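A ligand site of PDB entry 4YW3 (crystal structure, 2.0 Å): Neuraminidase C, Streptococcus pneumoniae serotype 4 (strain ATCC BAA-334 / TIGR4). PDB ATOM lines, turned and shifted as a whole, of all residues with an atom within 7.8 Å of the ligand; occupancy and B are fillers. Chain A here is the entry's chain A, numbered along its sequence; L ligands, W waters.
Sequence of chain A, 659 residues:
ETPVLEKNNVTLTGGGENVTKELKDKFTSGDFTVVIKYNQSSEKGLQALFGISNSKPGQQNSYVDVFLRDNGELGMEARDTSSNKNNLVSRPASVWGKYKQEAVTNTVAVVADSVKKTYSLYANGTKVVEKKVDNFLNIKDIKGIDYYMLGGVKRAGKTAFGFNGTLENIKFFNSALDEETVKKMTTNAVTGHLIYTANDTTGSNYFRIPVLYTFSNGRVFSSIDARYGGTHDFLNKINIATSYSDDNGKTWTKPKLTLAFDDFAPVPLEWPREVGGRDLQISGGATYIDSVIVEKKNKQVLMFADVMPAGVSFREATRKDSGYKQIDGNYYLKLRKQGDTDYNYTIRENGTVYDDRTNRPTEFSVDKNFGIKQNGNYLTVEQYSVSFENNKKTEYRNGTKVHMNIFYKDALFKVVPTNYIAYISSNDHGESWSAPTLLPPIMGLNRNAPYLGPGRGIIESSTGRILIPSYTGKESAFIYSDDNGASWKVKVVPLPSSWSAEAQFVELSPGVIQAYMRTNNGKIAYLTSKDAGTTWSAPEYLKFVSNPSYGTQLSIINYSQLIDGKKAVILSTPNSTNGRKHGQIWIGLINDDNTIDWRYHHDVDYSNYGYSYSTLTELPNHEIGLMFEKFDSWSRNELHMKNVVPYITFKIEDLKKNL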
ATOM      1  N   GLY A  45     -17.236  -8.493 -39.864  1.00  0.00           N
ATOM      2  CA  GLY A  45     -16.369  -9.523 -39.334  1.00  0.00           C
ATOM      3  C   GLY A  45     -15.714  -9.093 -38.037  1.00  0.00           C
ATOM      4  O   GLY A  45     -15.713  -7.921 -37.642  1.00  0.00           O
ATOM      5  N   LEU A  46     -15.144 -10.067 -37.378  1.00  0.00           N
ATOM      6  CA  LEU A  46     -14.359  -9.889 -36.183  1.00  0.00           C
ATOM      7  C   LEU A  46     -12.946  -9.466 -36.580  1.00  0.00           C
ATOM      8  O   LEU A  46     -12.254 -10.194 -37.288  1.00  0.00           O
ATOM      9  CB  LEU A  46     -14.366 -11.197 -35.375  1.00  0.00           C
ATOM     10  CG  LEU A  46     -13.448 -11.192 -34.124  1.00  0.00           C
ATOM     11  CD1 LEU A  46     -13.878 -10.101 -33.174  1.00  0.00           C
ATOM     12  CD2 LEU A  46     -13.495 -12.557 -33.482  1.00  0.00           C
ATOM     13  N   GLN A  47     -12.505  -8.308 -36.114  1.00  0.00           N
ATOM     14  CA  GLN A  47     -11.253  -7.738 -36.561  1.00  0.00           C
ATOM     15  C   GLN A  47     -10.345  -7.391 -35.402  1.00  0.00           C
ATOM     16  O   GLN A  47     -10.736  -6.722 -34.446  1.00  0.00           O
ATOM     17  CB  GLN A  47     -11.521  -6.486 -37.375  1.00  0.00           C
ATOM     18  CG  GLN A  47     -12.251  -6.740 -38.672  1.00  0.00           C
ATOM     19  CD  GLN A  47     -12.468  -5.446 -39.448  1.00  0.00           C
ATOM     20  OE1 GLN A  47     -11.647  -4.532 -39.404  1.00  0.00           O
ATOM     21  NE2 GLN A  47     -13.611  -5.372 -40.158  1.00  0.00           N
ATOM     22  N   GLN A  60      -3.040 -22.478 -31.608  1.00  0.00           N
ATOM     23  CA  GLN A  60      -3.949 -21.460 -32.062  1.00  0.00           C
ATOM     24  C   GLN A  60      -4.742 -20.796 -30.933  1.00  0.00           C
ATOM     25  O   GLN A  60      -5.284 -19.726 -31.145  1.00  0.00           O
ATOM     26  CB  GLN A  60      -4.846 -21.970 -33.203  1.00  0.00           C
ATOM     27  CG  GLN A  60      -5.771 -23.119 -32.894  1.00  0.00           C
ATOM     28  CD  GLN A  60      -5.111 -24.489 -32.942  1.00  0.00           C
ATOM     29  OE1 GLN A  60      -3.920 -24.629 -33.131  1.00  0.00           O
ATOM     30  NE2 GLN A  60      -5.897 -25.516 -32.742  1.00  0.00           N
ATOM     31  N   ASN A  61      -4.765 -21.374 -29.732  1.00  0.00           N
ATOM     32  CA  ASN A  61      -5.347 -20.712 -28.546  1.00  0.00           C
ATOM     33  C   ASN A  61      -4.337 -20.045 -27.603  1.00  0.00           C
ATOM     34  O   ASN A  61      -4.599 -19.840 -26.401  1.00  0.00           O
ATOM     35  CB  ASN A  61      -6.229 -21.735 -27.795  1.00  0.00           C
ATOM     36  CG  ASN A  61      -7.393 -22.204 -28.642  1.00  0.00           C
ATOM     37  OD1 ASN A  61      -7.811 -21.534 -29.601  1.00  0.00           O
ATOM     38  ND2 ASN A  61      -7.948 -23.332 -28.281  1.00  0.00           N
ATOM     39  N   TYR A  63      -2.758 -16.617 -27.648  1.00  0.00           N
ATOM     40  CA  TYR A  63      -2.649 -15.280 -28.147  1.00  0.00           C
ATOM     41  C   TYR A  63      -3.251 -14.217 -27.284  1.00  0.00           C
ATOM     42  O   TYR A  63      -4.068 -14.480 -26.401  1.00  0.00           O
ATOM     43  CB  TYR A  63      -3.253 -15.149 -29.560  1.00  0.00           C
ATOM     44  CG  TYR A  63      -4.745 -15.371 -29.664  1.00  0.00           C
ATOM     45  CD1 TYR A  63      -5.247 -16.628 -29.907  1.00  0.00           C
ATOM     46  CD2 TYR A  63      -5.639 -14.328 -29.560  1.00  0.00           C
ATOM     47  CE1 TYR A  63      -6.612 -16.859 -30.027  1.00  0.00           C
ATOM     48  CE2 TYR A  63      -7.007 -14.534 -29.658  1.00  0.00           C
ATOM     49  CZ  TYR A  63      -7.495 -15.792 -29.910  1.00  0.00           C
ATOM     50  OH  TYR A  63      -8.848 -16.066 -30.025  1.00  0.00           O
ATOM     51  N   ASP A  65      -5.001 -10.278 -28.133  1.00  0.00           N
ATOM     52  CA  ASP A  65      -5.435  -9.305 -29.124  1.00  0.00           C
ATOM     53  C   ASP A  65      -6.427  -8.306 -28.524  1.00  0.00           C
ATOM     54  O   ASP A  65      -6.933  -8.506 -27.403  1.00  0.00           O
ATOM     55  CB  ASP A  65      -6.001  -9.982 -30.395  1.00  0.00           C
ATOM     56  CG  ASP A  65      -7.373 -10.621 -30.233  1.00  0.00           C
ATOM     57  OD1 ASP A  65      -7.846 -10.785 -29.079  1.00  0.00           O
ATOM     58  OD2 ASP A  65      -8.020 -10.948 -31.304  1.00  0.00           O
ATOM     59  N   PHE A  67      -9.879  -6.498 -30.164  1.00  0.00           N
ATOM     60  CA  PHE A  67     -10.769  -6.724 -31.287  1.00  0.00           C
ATOM     61  C   PHE A  67     -11.942  -5.767 -31.326  1.00  0.00           C
ATOM     62  O   PHE A  67     -12.350  -5.224 -30.297  1.00  0.00           O
ATOM     63  CB  PHE A  67     -11.263  -8.179 -31.330  1.00  0.00           C
ATOM     64  CG  PHE A  67     -12.127  -8.586 -30.153  1.00  0.00           C
ATOM     65  CD1 PHE A  67     -13.479  -8.309 -30.141  1.00  0.00           C
ATOM     66  CD2 PHE A  67     -11.587  -9.287 -29.065  1.00  0.00           C
ATOM     67  CE1 PHE A  67     -14.280  -8.723 -29.090  1.00  0.00           C
ATOM     68  CE2 PHE A  67     -12.390  -9.704 -28.004  1.00  0.00           C
ATOM     69  CZ  PHE A  67     -13.725  -9.421 -28.020  1.00  0.00           C
ATOM     70  N   LEU A  68     -12.471  -5.659 -32.535  1.00  0.00           N
ATOM     71  CA  LEU A  68     -13.663  -4.892 -32.852  1.00  0.00           C
ATOM     72  C   LEU A  68     -14.680  -5.797 -33.537  1.00  0.00           C
ATOM     73  O   LEU A  68     -14.327  -6.589 -34.422  1.00  0.00           O
ATOM     74  CB  LEU A  68     -13.318  -3.802 -33.833  1.00  0.00           C
ATOM     75  CG  LEU A  68     -12.253  -2.792 -33.403  1.00  0.00           C
ATOM     76  CD1 LEU A  68     -11.917  -1.858 -34.556  1.00  0.00           C
ATOM     77  CD2 LEU A  68     -12.738  -2.007 -32.190  1.00  0.00           C
ATOM     78  N   ARG A  69     -15.949  -5.621 -33.168  1.00  0.00           N
ATOM     79  CA  ARG A  69     -17.044  -6.271 -33.885  1.00  0.00           C
ATOM     80  C   ARG A  69     -17.861  -5.248 -34.643  1.00  0.00           C
ATOM     81  O   ARG A  69     -17.746  -4.018 -34.424  1.00  0.00           O
ATOM     82  CB  ARG A  69     -17.963  -7.016 -32.937  1.00  0.00           C
ATOM     83  CG  ARG A  69     -17.283  -8.022 -32.040  1.00  0.00           C
ATOM     84  CD  ARG A  69     -18.350  -8.772 -31.275  1.00  0.00           C
ATOM     85  NE  ARG A  69     -17.799  -9.614 -30.227  1.00  0.00           N
ATOM     86  CZ  ARG A  69     -17.318 -10.853 -30.424  1.00  0.00           C
ATOM     87  NH1 ARG A  69     -17.293 -11.400 -31.655  1.00  0.00           N
ATOM     88  NH2 ARG A  69     -16.853 -11.543 -29.388  1.00  0.00           N
ATOM     89  N   GLU A  73     -18.723  -3.172 -30.424  1.00  0.00           N
ATOM     90  CA  GLU A  73     -18.097  -3.776 -29.255  1.00  0.00           C
ATOM     91  C   GLU A  73     -16.578  -3.748 -29.400  1.00  0.00           C
ATOM     92  O   GLU A  73     -16.038  -4.035 -30.469  1.00  0.00           O
ATOM     93  CB  GLU A  73     -18.521  -5.233 -29.064  1.00  0.00           C
ATOM     94  CG  GLU A  73     -17.885  -5.839 -27.816  1.00  0.00           C
ATOM     95  CD  GLU A  73     -18.549  -7.138 -27.429  1.00  0.00           C
ATOM     96  OE1 GLU A  73     -18.447  -8.112 -28.173  1.00  0.00           O
ATOM     97  OE2 GLU A  73     -19.144  -7.205 -26.363  1.00  0.00           O
ATOM     98  N   GLY A  75     -13.192  -5.333 -27.482  1.00  0.00           N
ATOM     99  CA  GLY A  75     -12.787  -6.379 -26.573  1.00  0.00           C
ATOM    100  C   GLY A  75     -11.323  -6.728 -26.664  1.00  0.00           C
ATOM    101  O   GLY A  75     -10.580  -6.170 -27.494  1.00  0.00           O
ATOM    102  N   MET A  76     -10.888  -7.592 -25.779  1.00  0.00           N
ATOM    103  CA  MET A  76      -9.572  -8.196 -25.845  1.00  0.00           C
ATOM    104  C   MET A  76      -9.646  -9.652 -25.448  1.00  0.00           C
ATOM    105  O   MET A  76     -10.506 -10.057 -24.636  1.00  0.00           O
ATOM    106  CB  MET A  76      -8.585  -7.456 -24.939  1.00  0.00           C
ATOM    107  CG  MET A  76      -8.895  -7.578 -23.471  1.00  0.00           C
ATOM    108  SD  MET A  76      -8.156  -9.029 -22.609  1.00  0.00           S
ATOM    109  CE  MET A  76      -6.485  -8.442 -22.664  1.00  0.00           C
ATOM    110  N   GLU A  77      -8.734 -10.439 -26.000  1.00  0.00           N
ATOM    111  CA  GLU A  77      -8.548 -11.825 -25.560  1.00  0.00           C
ATOM    112  C   GLU A  77      -7.099 -11.996 -25.074  1.00  0.00           C
ATOM    113  O   GLU A  77      -6.185 -11.311 -25.561  1.00  0.00           O
ATOM    114  CB  GLU A  77      -8.869 -12.861 -26.672  1.00  0.00           C
ATOM    115  CG  GLU A  77     -10.262 -12.762 -27.269  1.00  0.00           C
ATOM    116  CD  GLU A  77     -10.688 -14.021 -28.001  1.00  0.00           C
ATOM    117  OE1 GLU A  77     -11.111 -14.971 -27.325  1.00  0.00           O
ATOM    118  OE2 GLU A  77     -10.597 -14.086 -29.247  1.00  0.00           O
ATOM    119  N   ARG A  79      -5.193 -15.642 -24.066  1.00  0.00           N
ATOM    120  CA  ARG A  79      -5.422 -17.069 -24.039  1.00  0.00           C
ATOM    121  C   ARG A  79      -4.090 -17.841 -24.100  1.00  0.00           C
ATOM    122  O   ARG A  79      -3.167 -17.410 -24.789  1.00  0.00           O
ATOM    123  CB  ARG A  79      -6.230 -17.500 -25.229  1.00  0.00           C
ATOM    124  CG  ARG A  79      -7.507 -16.707 -25.404  1.00  0.00           C
ATOM    125  CD  ARG A  79      -8.261 -17.153 -26.647  1.00  0.00           C
ATOM    126  NE  ARG A  79      -8.803 -18.494 -26.469  1.00  0.00           N
ATOM    127  CZ  ARG A  79      -9.377 -19.213 -27.427  1.00  0.00           C
ATOM    128  NH1 ARG A  79      -9.525 -18.716 -28.662  1.00  0.00           N
ATOM    129  NH2 ARG A  79      -9.833 -20.423 -27.164  1.00  0.00           N
ATOM    130  N   ASN A  86      -8.476 -18.944 -20.840  1.00  0.00           N
ATOM    131  CA  ASN A  86      -9.065 -18.166 -21.913  1.00  0.00           C
ATOM    132  C   ASN A  86      -9.783 -16.963 -21.306  1.00  0.00           C
ATOM    133  O   ASN A  86     -10.807 -17.102 -20.681  1.00  0.00           O
ATOM    134  CB  ASN A  86     -10.055 -19.040 -22.680  1.00  0.00           C
ATOM    135  CG  ASN A  86      -9.408 -20.301 -23.214  1.00  0.00           C
ATOM    136  OD1 ASN A  86      -8.634 -20.257 -24.170  1.00  0.00           O
ATOM    137  ND2 ASN A  86      -9.677 -21.404 -22.570  1.00  0.00           N
ATOM    138  N   ASN A  87      -9.178 -15.792 -21.450  1.00  0.00           N
ATOM    139  CA  ASN A  87      -9.703 -14.574 -20.881  1.00  0.00           C
ATOM    140  C   ASN A  87     -10.292 -13.774 -22.011  1.00  0.00           C
ATOM    141  O   ASN A  87      -9.654 -13.631 -23.046  1.00  0.00           O
ATOM    142  CB  ASN A  87      -8.603 -13.780 -20.143  1.00  0.00           C
ATOM    143  CG  ASN A  87      -7.992 -14.567 -18.991  1.00  0.00           C
ATOM    144  OD1 ASN A  87      -8.691 -14.934 -18.068  1.00  0.00           O
ATOM    145  ND2 ASN A  87      -6.707 -14.849 -19.062  1.00  0.00           N
ATOM    146  N   LEU A  88     -11.500 -13.250 -21.795  1.00  0.00           N
ATOM    147  CA  LEU A  88     -12.124 -12.337 -22.748  1.00  0.00           C
ATOM    148  C   LEU A  88     -12.761 -11.210 -21.939  1.00  0.00           C
ATOM    149  O   LEU A  88     -13.554 -11.473 -21.063  1.00  0.00           O
ATOM    150  CB  LEU A  88     -13.149 -13.044 -23.600  1.00  0.00           C
ATOM    151  CG  LEU A  88     -13.676 -12.207 -24.792  1.00  0.00           C
ATOM    152  CD1 LEU A  88     -14.211 -13.097 -25.919  1.00  0.00           C
ATOM    153  CD2 LEU A  88     -14.800 -11.281 -24.359  1.00  0.00           C
ATOM    154  N   SER A  90     -14.491  -7.289 -22.448  1.00  0.00           N
ATOM    155  CA  SER A  90     -15.084  -6.437 -23.477  1.00  0.00           C
ATOM    156  C   SER A  90     -16.196  -5.544 -22.913  1.00  0.00           C
ATOM    157  O   SER A  90     -16.660  -5.738 -21.792  1.00  0.00           O
ATOM    158  CB  SER A  90     -15.657  -7.293 -24.586  1.00  0.00           C
ATOM    159  OG  SER A  90     -16.819  -7.922 -24.127  1.00  0.00           O
ATOM    160  N   ARG A 155      -2.449 -17.484 -36.350  1.00  0.00           N
ATOM    161  CA  ARG A 155      -2.878 -18.746 -35.738  1.00  0.00           C
ATOM    162  C   ARG A 155      -2.588 -19.871 -36.695  1.00  0.00           C
ATOM    163  O   ARG A 155      -3.126 -19.875 -37.801  1.00  0.00           O
ATOM    164  CB  ARG A 155      -4.366 -18.720 -35.430  1.00  0.00           C
ATOM    165  CG  ARG A 155      -4.762 -17.567 -34.512  1.00  0.00           C
ATOM    166  CD  ARG A 155      -6.248 -17.565 -34.259  1.00  0.00           C
ATOM    167  NE  ARG A 155      -6.672 -18.525 -33.255  1.00  0.00           N
ATOM    168  CZ  ARG A 155      -7.933 -18.847 -32.987  1.00  0.00           C
ATOM    169  NH1 ARG A 155      -8.962 -18.323 -33.696  1.00  0.00           N
ATOM    170  NH2 ARG A 155      -8.202 -19.673 -31.984  1.00  0.00           N
ATOM    171  N   ALA A 160      -5.701 -14.621 -38.856  1.00  0.00           N
ATOM    172  CA  ALA A 160      -7.073 -14.589 -38.369  1.00  0.00           C
ATOM    173  C   ALA A 160      -7.472 -13.150 -38.000  1.00  0.00           C
ATOM    174  O   ALA A 160      -6.622 -12.316 -37.620  1.00  0.00           O
ATOM    175  CB  ALA A 160      -7.224 -15.513 -37.157  1.00  0.00           C
ATOM    176  N   PHE A 161      -8.779 -12.886 -38.120  1.00  0.00           N
ATOM    177  CA  PHE A 161      -9.409 -11.668 -37.636  1.00  0.00           C
ATOM    178  C   PHE A 161      -8.820 -10.473 -38.349  1.00  0.00           C
ATOM    179  O   PHE A 161      -8.508  -9.456 -37.713  1.00  0.00           O
ATOM    180  CB  PHE A 161      -9.210 -11.484 -36.107  1.00  0.00           C
ATOM    181  CG  PHE A 161      -9.460 -12.729 -35.279  1.00  0.00           C
ATOM    182  CD1 PHE A 161     -10.621 -13.495 -35.460  1.00  0.00           C
ATOM    183  CD2 PHE A 161      -8.566 -13.112 -34.275  1.00  0.00           C
ATOM    184  CE1 PHE A 161     -10.842 -14.624 -34.664  1.00  0.00           C
ATOM    185  CE2 PHE A 161      -8.776 -14.234 -33.485  1.00  0.00           C
ATOM    186  CZ  PHE A 161      -9.930 -14.984 -33.668  1.00  0.00           C
HETATM  187  C1  LIG L   1     -11.826 -19.287 -31.541  1.00  0.00           C
HETATM  188  C2  LIG L   1     -13.221 -19.125 -31.000  1.00  0.00           C
HETATM  189  C3  LIG L   1     -13.240 -18.666 -29.530  1.00  0.00           C
HETATM  190  C4  LIG L   1     -12.768 -17.213 -29.414  1.00  0.00           C
HETATM  191  C5  LIG L   1     -13.689 -16.343 -30.248  1.00  0.00           C
HETATM  192  C6  LIG L   1     -13.615 -16.818 -31.705  1.00  0.00           C
HETATM  193  C7  LIG L   1     -14.554 -16.129 -32.690  1.00  0.00           C
HETATM  194  C8  LIG L   1     -14.644 -16.906 -33.989  1.00  0.00           C
HETATM  195  C9  LIG L   1     -15.513 -16.229 -35.046  1.00  0.00           C
HETATM  196  C10 LIG L   1     -14.113 -13.895 -30.084  1.00  0.00           C
HETATM  197  C11 LIG L   1     -13.479 -12.558 -29.814  1.00  0.00           C
HETATM  198  N1  LIG L   1     -13.288 -14.942 -30.135  1.00  0.00           N
HETATM  199  O1  LIG L   1     -11.533 -18.773 -32.635  1.00  0.00           O
HETATM  200  O2  LIG L   1     -11.004 -19.949 -30.908  1.00  0.00           O
HETATM  201  O3  LIG L   1     -13.845 -20.400 -31.150  1.00  0.00           O
HETATM  202  O4  LIG L   1     -12.731 -16.760 -28.048  1.00  0.00           O
HETATM  203  O5  LIG L   1     -13.961 -18.203 -31.801  1.00  0.00           O
HETATM  204  O6  LIG L   1     -15.854 -16.068 -32.111  1.00  0.00           O
HETATM  205  O7  LIG L   1     -13.302 -17.119 -34.452  1.00  0.00           O
HETATM  206  O8  LIG L   1     -14.793 -15.160 -35.671  1.00  0.00           O
HETATM  207  O9  LIG L   1     -15.325 -13.978 -30.243  1.00  0.00           O
HETATM  208  O   HOH W   1     -11.382 -21.817 -29.095  1.00  0.00           O
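OE1 of Glu 77 is in hydrogen-bond range of O4 of the ligand, 2.5 Å away.
An oxygen (O1) of the ligand is in salt-bridge range of the guanidinium group (NH1) of Arg 155, at 2.8 Å.
O2 of the ligand lies within salt-bridge range of NH1 of Arg 79 (3.0 Å).
The guanidinium group (NH2) of Arg 69 lies within hydrogen-bond range of an oxygen (O9) of the ligand, at 3.0 Å.
Merely in contact with the ligand: Leu 46 (3.6 Å), Asn 61 (3.8 Å), Phe 67 (3.6 Å), Leu 88 (3.9997 Å) and Phe 161 (3.5 Å).
Hydrophobic or aromatic side chains that line the ligand: Leu 46, Phe 67, Leu 88 and Phe 161.
Nine residues have an atom within 4 Å of the ligand: Leu 46, Asn 61, Phe 67, Arg 69, Glu 77, Arg 79, Leu 88, Arg 155 and Phe 161.
The side-chain hydroxyl (OH) of Tyr 63 is in hydrogen-bond range of the side-chain carboxylate (OE2) of Glu 77 (2.8 Å).
N of Glu 77 lies within hydrogen-bond range of O of Asp 65 (3.0 Å).
The side-chain amide oxygen (OD1) of Asn 61 is in hydrogen-bond range of the guanidinium group (NH2) of Arg 155 (3.0 Å).
NE of Arg 155 sits at hydrogen-bond distance from O of Gln 60, 2.8 Å away.
The guanidinium group (NH2) of Arg 79 sits at hydrogen-bond distance from the side-chain amide oxygen (OD1) of Asn 61 (3.4 Å).
The backbone NH of Arg 79 sits at hydrogen-bond distance from the backbone carbonyl oxygen of Tyr 63, 2.8 Å away.
NE of Arg 79 sits at hydrogen-bond distance from OD1 of Asn 86 (2.9 Å).
The side-chain carboxylate (OE1) of Glu 73 lies within salt-bridge range of the guanidinium group (NE) of Arg 69, 2.6 Å away.
Water W1 lies within hydrogen-bond range of O2 of the ligand (2.6 Å) and NH2 of Arg 79 (2.8 Å).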
